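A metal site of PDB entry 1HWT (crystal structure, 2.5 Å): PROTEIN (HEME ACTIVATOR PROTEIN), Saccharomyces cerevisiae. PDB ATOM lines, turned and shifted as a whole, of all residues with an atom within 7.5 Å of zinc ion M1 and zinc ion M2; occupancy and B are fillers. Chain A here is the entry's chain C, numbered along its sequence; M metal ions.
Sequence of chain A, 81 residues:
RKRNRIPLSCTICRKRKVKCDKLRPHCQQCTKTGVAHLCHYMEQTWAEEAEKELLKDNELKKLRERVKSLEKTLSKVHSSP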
ATOM      1  N   LEU A   8     -33.629 -14.842  15.355  1.00  0.00           N
ATOM      2  CA  LEU A   8     -33.211 -15.006  13.968  1.00  0.00           C
ATOM      3  C   LEU A   8     -31.768 -14.604  13.700  1.00  0.00           C
ATOM      4  O   LEU A   8     -31.190 -14.981  12.682  1.00  0.00           O
ATOM      5  CB  LEU A   8     -34.132 -14.204  13.062  1.00  0.00           C
ATOM      6  CG  LEU A   8     -35.608 -14.556  13.222  1.00  0.00           C
ATOM      7  CD1 LEU A   8     -36.443 -13.646  12.350  1.00  0.00           C
ATOM      8  CD2 LEU A   8     -35.822 -15.998  12.836  1.00  0.00           C
ATOM      9  N   SER A   9     -31.184 -13.816  14.607  1.00  0.00           N
ATOM     10  CA  SER A   9     -29.799 -13.386  14.441  1.00  0.00           C
ATOM     11  C   SER A   9     -28.884 -14.406  15.083  1.00  0.00           C
ATOM     12  O   SER A   9     -29.192 -14.945  16.151  1.00  0.00           O
ATOM     13  CB  SER A   9     -29.590 -12.019  15.093  1.00  0.00           C
ATOM     14  OG  SER A   9     -30.531 -11.090  14.620  1.00  0.00           O
ATOM     15  N   CYS A  10     -27.748 -14.678  14.431  1.00  0.00           N
ATOM     16  CA  CYS A  10     -26.777 -15.627  14.956  1.00  0.00           C
ATOM     17  C   CYS A  10     -26.344 -15.206  16.366  1.00  0.00           C
ATOM     18  O   CYS A  10     -26.308 -14.024  16.678  1.00  0.00           O
ATOM     19  CB  CYS A  10     -25.565 -15.734  14.024  1.00  0.00           C
ATOM     20  SG  CYS A  10     -24.351 -14.377  14.125  1.00  0.00           S
ATOM     21  N   THR A  11     -26.051 -16.185  17.202  1.00  0.00           N
ATOM     22  CA  THR A  11     -25.654 -15.926  18.567  1.00  0.00           C
ATOM     23  C   THR A  11     -24.527 -14.904  18.724  1.00  0.00           C
ATOM     24  O   THR A  11     -24.550 -14.097  19.640  1.00  0.00           O
ATOM     25  CB  THR A  11     -25.244 -17.233  19.296  1.00  0.00           C
ATOM     26  OG1 THR A  11     -24.415 -18.031  18.441  1.00  0.00           O
ATOM     27  CG2 THR A  11     -26.472 -18.020  19.677  1.00  0.00           C
ATOM     28  N   ILE A  12     -23.539 -14.929  17.832  1.00  0.00           N
ATOM     29  CA  ILE A  12     -22.434 -14.003  17.950  1.00  0.00           C
ATOM     30  C   ILE A  12     -22.848 -12.557  17.764  1.00  0.00           C
ATOM     31  O   ILE A  12     -22.453 -11.693  18.543  1.00  0.00           O
ATOM     32  CB  ILE A  12     -21.303 -14.323  16.951  1.00  0.00           C
ATOM     33  CG1 ILE A  12     -20.716 -15.707  17.246  1.00  0.00           C
ATOM     34  CG2 ILE A  12     -20.230 -13.254  17.008  1.00  0.00           C
ATOM     35  CD1 ILE A  12     -20.172 -15.849  18.635  1.00  0.00           C
ATOM     36  N   CYS A  13     -23.634 -12.278  16.723  1.00  0.00           N
ATOM     37  CA  CYS A  13     -24.096 -10.913  16.453  1.00  0.00           C
ATOM     38  C   CYS A  13     -24.959 -10.444  17.600  1.00  0.00           C
ATOM     39  O   CYS A  13     -25.004  -9.249  17.917  1.00  0.00           O
ATOM     40  CB  CYS A  13     -24.908 -10.851  15.172  1.00  0.00           C
ATOM     41  SG  CYS A  13     -23.888 -10.795  13.671  1.00  0.00           S
ATOM     42  N   ARG A  14     -25.666 -11.383  18.201  1.00  0.00           N
ATOM     43  CA  ARG A  14     -26.505 -11.097  19.343  1.00  0.00           C
ATOM     44  C   ARG A  14     -25.602 -10.575  20.453  1.00  0.00           C
ATOM     45  O   ARG A  14     -25.817  -9.488  20.960  1.00  0.00           O
ATOM     46  CB  ARG A  14     -27.203 -12.369  19.811  1.00  0.00           C
ATOM     47  CG  ARG A  14     -28.692 -12.220  20.036  1.00  0.00           C
ATOM     48  CD  ARG A  14     -29.487 -13.091  19.087  1.00  0.00           C
ATOM     49  NE  ARG A  14     -29.339 -14.514  19.407  1.00  0.00           N
ATOM     50  CZ  ARG A  14     -29.648 -15.077  20.576  1.00  0.00           C
ATOM     51  NH1 ARG A  14     -30.141 -14.318  21.550  1.00  0.00           N
ATOM     52  NH2 ARG A  14     -29.465 -16.379  20.761  1.00  0.00           N
ATOM     53  N   VAL A  18     -24.687  -6.281  17.189  1.00  0.00           N
ATOM     54  CA  VAL A  18     -24.617  -5.665  15.869  1.00  0.00           C
ATOM     55  C   VAL A  18     -25.705  -6.277  15.009  1.00  0.00           C
ATOM     56  O   VAL A  18     -26.272  -7.285  15.374  1.00  0.00           O
ATOM     57  CB  VAL A  18     -23.263  -5.912  15.208  1.00  0.00           C
ATOM     58  CG1 VAL A  18     -22.176  -5.272  16.037  1.00  0.00           C
ATOM     59  CG2 VAL A  18     -23.003  -7.380  15.094  1.00  0.00           C
ATOM     60  N   LYS A  19     -26.011  -5.688  13.871  1.00  0.00           N
ATOM     61  CA  LYS A  19     -27.049  -6.213  13.004  1.00  0.00           C
ATOM     62  C   LYS A  19     -26.600  -7.464  12.240  1.00  0.00           C
ATOM     63  O   LYS A  19     -25.552  -7.464  11.584  1.00  0.00           O
ATOM     64  CB  LYS A  19     -27.499  -5.133  12.020  1.00  0.00           C
ATOM     65  CG  LYS A  19     -28.239  -5.643  10.794  1.00  0.00           C
ATOM     66  CD  LYS A  19     -29.738  -5.453  10.948  1.00  0.00           C
ATOM     67  CE  LYS A  19     -30.294  -4.506   9.877  1.00  0.00           C
ATOM     68  NZ  LYS A  19     -29.861  -3.067  10.072  1.00  0.00           N
ATOM     69  N   CYS A  20     -27.408  -8.521  12.321  1.00  0.00           N
ATOM     70  CA  CYS A  20     -27.112  -9.767  11.627  1.00  0.00           C
ATOM     71  C   CYS A  20     -27.828  -9.808  10.262  1.00  0.00           C
ATOM     72  O   CYS A  20     -29.027  -9.549  10.179  1.00  0.00           O
ATOM     73  CB  CYS A  20     -27.558 -10.966  12.474  1.00  0.00           C
ATOM     74  SG  CYS A  20     -26.931 -12.567  11.881  1.00  0.00           S
ATOM     75  N   ASP A  21     -27.091 -10.116   9.202  1.00  0.00           N
ATOM     76  CA  ASP A  21     -27.701 -10.198   7.881  1.00  0.00           C
ATOM     77  C   ASP A  21     -28.408 -11.534   7.698  1.00  0.00           C
ATOM     78  O   ASP A  21     -28.939 -11.820   6.626  1.00  0.00           O
ATOM     79  CB  ASP A  21     -26.660 -10.033   6.793  1.00  0.00           C
ATOM     80  CG  ASP A  21     -25.408 -10.770   7.109  1.00  0.00           C
ATOM     81  OD1 ASP A  21     -24.644 -10.256   7.952  1.00  0.00           O
ATOM     82  OD2 ASP A  21     -25.177 -11.862   6.538  1.00  0.00           O
ATOM     83  N   LYS A  22     -28.388 -12.364   8.743  1.00  0.00           N
ATOM     84  CA  LYS A  22     -29.046 -13.666   8.741  1.00  0.00           C
ATOM     85  C   LYS A  22     -28.779 -14.568   7.549  1.00  0.00           C
ATOM     86  O   LYS A  22     -29.610 -15.412   7.203  1.00  0.00           O
ATOM     87  CB  LYS A  22     -30.551 -13.459   8.897  1.00  0.00           C
ATOM     88  CG  LYS A  22     -30.982 -12.855  10.233  1.00  0.00           C
ATOM     89  CD  LYS A  22     -31.747 -11.549  10.048  1.00  0.00           C
ATOM     90  CE  LYS A  22     -32.224 -10.981  11.389  1.00  0.00           C
ATOM     91  NZ  LYS A  22     -31.986  -9.494  11.517  1.00  0.00           N
ATOM     92  N   LEU A  23     -27.614 -14.420   6.934  1.00  0.00           N
ATOM     93  CA  LEU A  23     -27.240 -15.232   5.780  1.00  0.00           C
ATOM     94  C   LEU A  23     -26.653 -16.560   6.228  1.00  0.00           C
ATOM     95  O   LEU A  23     -25.950 -16.616   7.224  1.00  0.00           O
ATOM     96  CB  LEU A  23     -26.241 -14.482   4.891  1.00  0.00           C
ATOM     97  CG  LEU A  23     -26.718 -13.087   4.422  1.00  0.00           C
ATOM     98  CD1 LEU A  23     -25.651 -12.488   3.504  1.00  0.00           C
ATOM     99  CD2 LEU A  23     -28.074 -13.163   3.698  1.00  0.00           C
ATOM    100  N   PRO A  25     -24.514 -20.297   5.245  1.00  0.00           N
ATOM    101  CA  PRO A  25     -24.534 -20.996   6.532  1.00  0.00           C
ATOM    102  C   PRO A  25     -24.094 -20.089   7.662  1.00  0.00           C
ATOM    103  O   PRO A  25     -24.487 -20.272   8.818  1.00  0.00           O
ATOM    104  CB  PRO A  25     -23.544 -22.132   6.323  1.00  0.00           C
ATOM    105  CG  PRO A  25     -22.552 -21.573   5.353  1.00  0.00           C
ATOM    106  CD  PRO A  25     -23.367 -20.699   4.418  1.00  0.00           C
ATOM    107  N   HIS A  26     -23.282 -19.098   7.312  1.00  0.00           N
ATOM    108  CA  HIS A  26     -22.774 -18.128   8.275  1.00  0.00           C
ATOM    109  C   HIS A  26     -22.970 -16.735   7.737  1.00  0.00           C
ATOM    110  O   HIS A  26     -22.785 -16.504   6.534  1.00  0.00           O
ATOM    111  CB  HIS A  26     -21.286 -18.350   8.518  1.00  0.00           C
ATOM    112  CG  HIS A  26     -20.925 -19.788   8.733  1.00  0.00           C
ATOM    113  ND1 HIS A  26     -21.419 -20.528   9.777  1.00  0.00           N
ATOM    114  CD2 HIS A  26     -20.109 -20.617   8.036  1.00  0.00           C
ATOM    115  CE1 HIS A  26     -20.939 -21.755   9.717  1.00  0.00           C
ATOM    116  NE2 HIS A  26     -20.135 -21.831   8.677  1.00  0.00           N
ATOM    117  N   CYS A  27     -23.332 -15.813   8.622  1.00  0.00           N
ATOM    118  CA  CYS A  27     -23.579 -14.426   8.249  1.00  0.00           C
ATOM    119  C   CYS A  27     -22.278 -13.725   7.888  1.00  0.00           C
ATOM    120  O   CYS A  27     -21.197 -14.163   8.286  1.00  0.00           O
ATOM    121  CB  CYS A  27     -24.305 -13.702   9.377  1.00  0.00           C
ATOM    122  SG  CYS A  27     -23.269 -13.298  10.808  1.00  0.00           S
ATOM    123  N   GLN A  28     -22.381 -12.637   7.124  1.00  0.00           N
ATOM    124  CA  GLN A  28     -21.196 -11.891   6.701  1.00  0.00           C
ATOM    125  C   GLN A  28     -20.488 -11.151   7.826  1.00  0.00           C
ATOM    126  O   GLN A  28     -19.320 -10.818   7.705  1.00  0.00           O
ATOM    127  CB  GLN A  28     -21.565 -10.909   5.591  1.00  0.00           C
ATOM    128  CG  GLN A  28     -21.469 -11.492   4.201  1.00  0.00           C
ATOM    129  CD  GLN A  28     -20.071 -11.963   3.856  1.00  0.00           C
ATOM    130  OE1 GLN A  28     -19.902 -12.925   3.078  1.00  0.00           O
ATOM    131  NE2 GLN A  28     -19.062 -11.309   4.420  1.00  0.00           N
ATOM    132  N   GLN A  29     -21.185 -10.876   8.923  1.00  0.00           N
ATOM    133  CA  GLN A  29     -20.561 -10.179  10.038  1.00  0.00           C
ATOM    134  C   GLN A  29     -19.507 -11.071  10.654  1.00  0.00           C
ATOM    135  O   GLN A  29     -18.397 -10.635  10.907  1.00  0.00           O
ATOM    136  CB  GLN A  29     -21.605  -9.827  11.091  1.00  0.00           C
ATOM    137  CG  GLN A  29     -21.820  -8.336  11.257  1.00  0.00           C
ATOM    138  CD  GLN A  29     -22.970  -7.854  10.414  1.00  0.00           C
ATOM    139  OE1 GLN A  29     -23.516  -8.627   9.609  1.00  0.00           O
ATOM    140  NE2 GLN A  29     -23.347  -6.596  10.588  1.00  0.00           N
ATOM    141  N   CYS A  30     -19.870 -12.319  10.902  1.00  0.00           N
ATOM    142  CA  CYS A  30     -18.942 -13.282  11.462  1.00  0.00           C
ATOM    143  C   CYS A  30     -17.888 -13.538  10.414  1.00  0.00           C
ATOM    144  O   CYS A  30     -16.703 -13.604  10.709  1.00  0.00           O
ATOM    145  CB  CYS A  30     -19.652 -14.596  11.769  1.00  0.00           C
ATOM    146  SG  CYS A  30     -20.652 -14.621  13.285  1.00  0.00           S
ATOM    147  N   THR A  31     -18.326 -13.708   9.164  1.00  0.00           N
ATOM    148  CA  THR A  31     -17.384 -13.996   8.098  1.00  0.00           C
ATOM    149  C   THR A  31     -16.285 -12.949   8.058  1.00  0.00           C
ATOM    150  O   THR A  31     -15.102 -13.264   8.145  1.00  0.00           O
ATOM    151  CB  THR A  31     -18.078 -14.031   6.743  1.00  0.00           C
ATOM    152  OG1 THR A  31     -18.870 -15.215   6.636  1.00  0.00           O
ATOM    153  CG2 THR A  31     -17.061 -14.009   5.634  1.00  0.00           C
ATOM    154  N   THR A  33     -15.280 -10.823  10.257  1.00  0.00           N
ATOM    155  CA  THR A  33     -14.458 -10.680  11.453  1.00  0.00           C
ATOM    156  C   THR A  33     -13.618 -11.923  11.643  1.00  0.00           C
ATOM    157  O   THR A  33     -12.861 -12.035  12.598  1.00  0.00           O
ATOM    158  CB  THR A  33     -15.292 -10.458  12.743  1.00  0.00           C
ATOM    159  OG1 THR A  33     -16.454 -11.294  12.734  1.00  0.00           O
ATOM    160  CG2 THR A  33     -15.736  -9.012  12.839  1.00  0.00           C
ATOM    161  N   VAL A  35     -14.755 -15.086  12.181  1.00  0.00           N
ATOM    162  CA  VAL A  35     -15.280 -16.065  13.116  1.00  0.00           C
ATOM    163  C   VAL A  35     -16.436 -16.905  12.577  1.00  0.00           C
ATOM    164  O   VAL A  35     -17.256 -17.404  13.346  1.00  0.00           O
ATOM    165  CB  VAL A  35     -15.715 -15.375  14.441  1.00  0.00           C
ATOM    166  CG1 VAL A  35     -14.488 -14.858  15.166  1.00  0.00           C
ATOM    167  CG2 VAL A  35     -16.664 -14.236  14.163  1.00  0.00           C
ATOM    168  N   ALA A  36     -16.478 -17.078  11.261  1.00  0.00           N
ATOM    169  CA  ALA A  36     -17.536 -17.852  10.611  1.00  0.00           C
ATOM    170  C   ALA A  36     -17.694 -19.237  11.200  1.00  0.00           C
ATOM    171  O   ALA A  36     -18.793 -19.779  11.249  1.00  0.00           O
ATOM    172  CB  ALA A  36     -17.267 -17.960   9.131  1.00  0.00           C
ATOM    173  N   LEU A  38     -17.682 -19.965  14.065  1.00  0.00           N
ATOM    174  CA  LEU A  38     -18.381 -19.865  15.335  1.00  0.00           C
ATOM    175  C   LEU A  38     -19.782 -19.324  15.118  1.00  0.00           C
ATOM    176  O   LEU A  38     -20.540 -19.140  16.062  1.00  0.00           O
ATOM    177  CB  LEU A  38     -17.636 -18.939  16.295  1.00  0.00           C
ATOM    178  CG  LEU A  38     -16.193 -19.269  16.688  1.00  0.00           C
ATOM    179  CD1 LEU A  38     -15.751 -18.291  17.753  1.00  0.00           C
ATOM    180  CD2 LEU A  38     -16.088 -20.697  17.184  1.00  0.00           C
ATOM    181  N   CYS A  39     -20.123 -19.087  13.864  1.00  0.00           N
ATOM    182  CA  CYS A  39     -21.440 -18.541  13.547  1.00  0.00           C
ATOM    183  C   CYS A  39     -22.476 -19.618  13.402  1.00  0.00           C
ATOM    184  O   CYS A  39     -22.354 -20.482  12.546  1.00  0.00           O
ATOM    185  CB  CYS A  39     -21.413 -17.768  12.235  1.00  0.00           C
ATOM    186  SG  CYS A  39     -23.051 -17.111  11.821  1.00  0.00           S
ATOM    187  N   HIS A  40     -23.488 -19.565  14.246  1.00  0.00           N
ATOM    188  CA  HIS A  40     -24.556 -20.546  14.189  1.00  0.00           C
ATOM    189  C   HIS A  40     -25.852 -19.907  14.636  1.00  0.00           C
ATOM    190  O   HIS A  40     -25.840 -18.927  15.391  1.00  0.00           O
ATOM    191  CB  HIS A  40     -24.213 -21.769  15.053  1.00  0.00           C
ATOM    192  CG  HIS A  40     -24.145 -21.493  16.520  1.00  0.00           C
ATOM    193  ND1 HIS A  40     -25.222 -21.630  17.363  1.00  0.00           N
ATOM    194  CD2 HIS A  40     -23.103 -21.111  17.298  1.00  0.00           C
ATOM    195  CE1 HIS A  40     -24.847 -21.358  18.599  1.00  0.00           C
ATOM    196  NE2 HIS A  40     -23.567 -21.040  18.592  1.00  0.00           N
ATOM    197  N   TYR A  41     -26.960 -20.452  14.148  1.00  0.00           N
ATOM    198  CA  TYR A  41     -28.285 -19.958  14.478  1.00  0.00           C
ATOM    199  C   TYR A  41     -28.999 -20.966  15.338  1.00  0.00           C
ATOM    200  O   TYR A  41     -28.779 -22.171  15.220  1.00  0.00           O
ATOM    201  CB  TYR A  41     -29.084 -19.749  13.200  1.00  0.00           C
ATOM    202  CG  TYR A  41     -28.460 -18.748  12.267  1.00  0.00           C
ATOM    203  CD1 TYR A  41     -27.518 -19.141  11.307  1.00  0.00           C
ATOM    204  CD2 TYR A  41     -28.803 -17.397  12.338  1.00  0.00           C
ATOM    205  CE1 TYR A  41     -26.921 -18.201  10.457  1.00  0.00           C
ATOM    206  CE2 TYR A  41     -28.227 -16.460  11.495  1.00  0.00           C
ATOM    207  CZ  TYR A  41     -27.299 -16.867  10.557  1.00  0.00           C
ATOM    208  OH  TYR A  41     -26.772 -15.928   9.698  1.00  0.00           O
HETATM  209 ZN    ZN M   1     -22.866 -14.924  12.512  1.00  0.00          ZN
HETATM  210 ZN    ZN M   2     -24.626 -12.635  12.511  1.00  0.00          ZN
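The backbone NH (N) of Gln 29 sits close to the side-chain sulfur (SG) of Cys 27 (3.7 Å).
The backbone carbonyl oxygen (O) of Cys 20 is in hydrogen-bond range of the side-chain amino group (NZ) of Lys 22, at 3.2 Å.
OG1 of Thr 33 lies within hydrogen-bond range of O of Cys 30, at 3.1 Å.
ND1 of His 26 sits at hydrogen-bond distance from O of Cys 39, 2.9 Å away.
OG1 of Thr 31 is in hydrogen-bond range of O of Cys 27, at 3.0 Å.
O of Cys 13 sits at hydrogen-bond distance from N of Val 18, at 3.1 Å.
The backbone carbonyl oxygen (O) of Cys 30 is in hydrogen-bond range of the backbone NH (N) of Val 35, at 2.9 Å.
Zinc ion M1 is bound by the side-chain sulfur (SG) of Cys 10, the side-chain sulfur (SG) of Cys 39, the side-chain sulfur (SG) of Cys 30 and the side-chain sulfur (SG) of Cys 27.
The nearest printed residue that does not touch zinc ion M2 is Gln 29 (4.4 Å).
Four residues have an atom within 4 Å of zinc ion M1: Cys 10, Cys 27, Cys 30 and Cys 39.
The nearest printed residue that does not touch zinc ion M1 is Cys 13 (4.4 Å).
Zinc ion M2 is bound by SG of Cys 27, 2.3 Å away.
Zinc ion M2 is bound by SG of Cys 13, at 2.3 Å.
SG of Cys 20 binds zinc ion M2 (2.4 Å).
SG of Cys 10 is bound to zinc ion M2 (2.4 Å).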
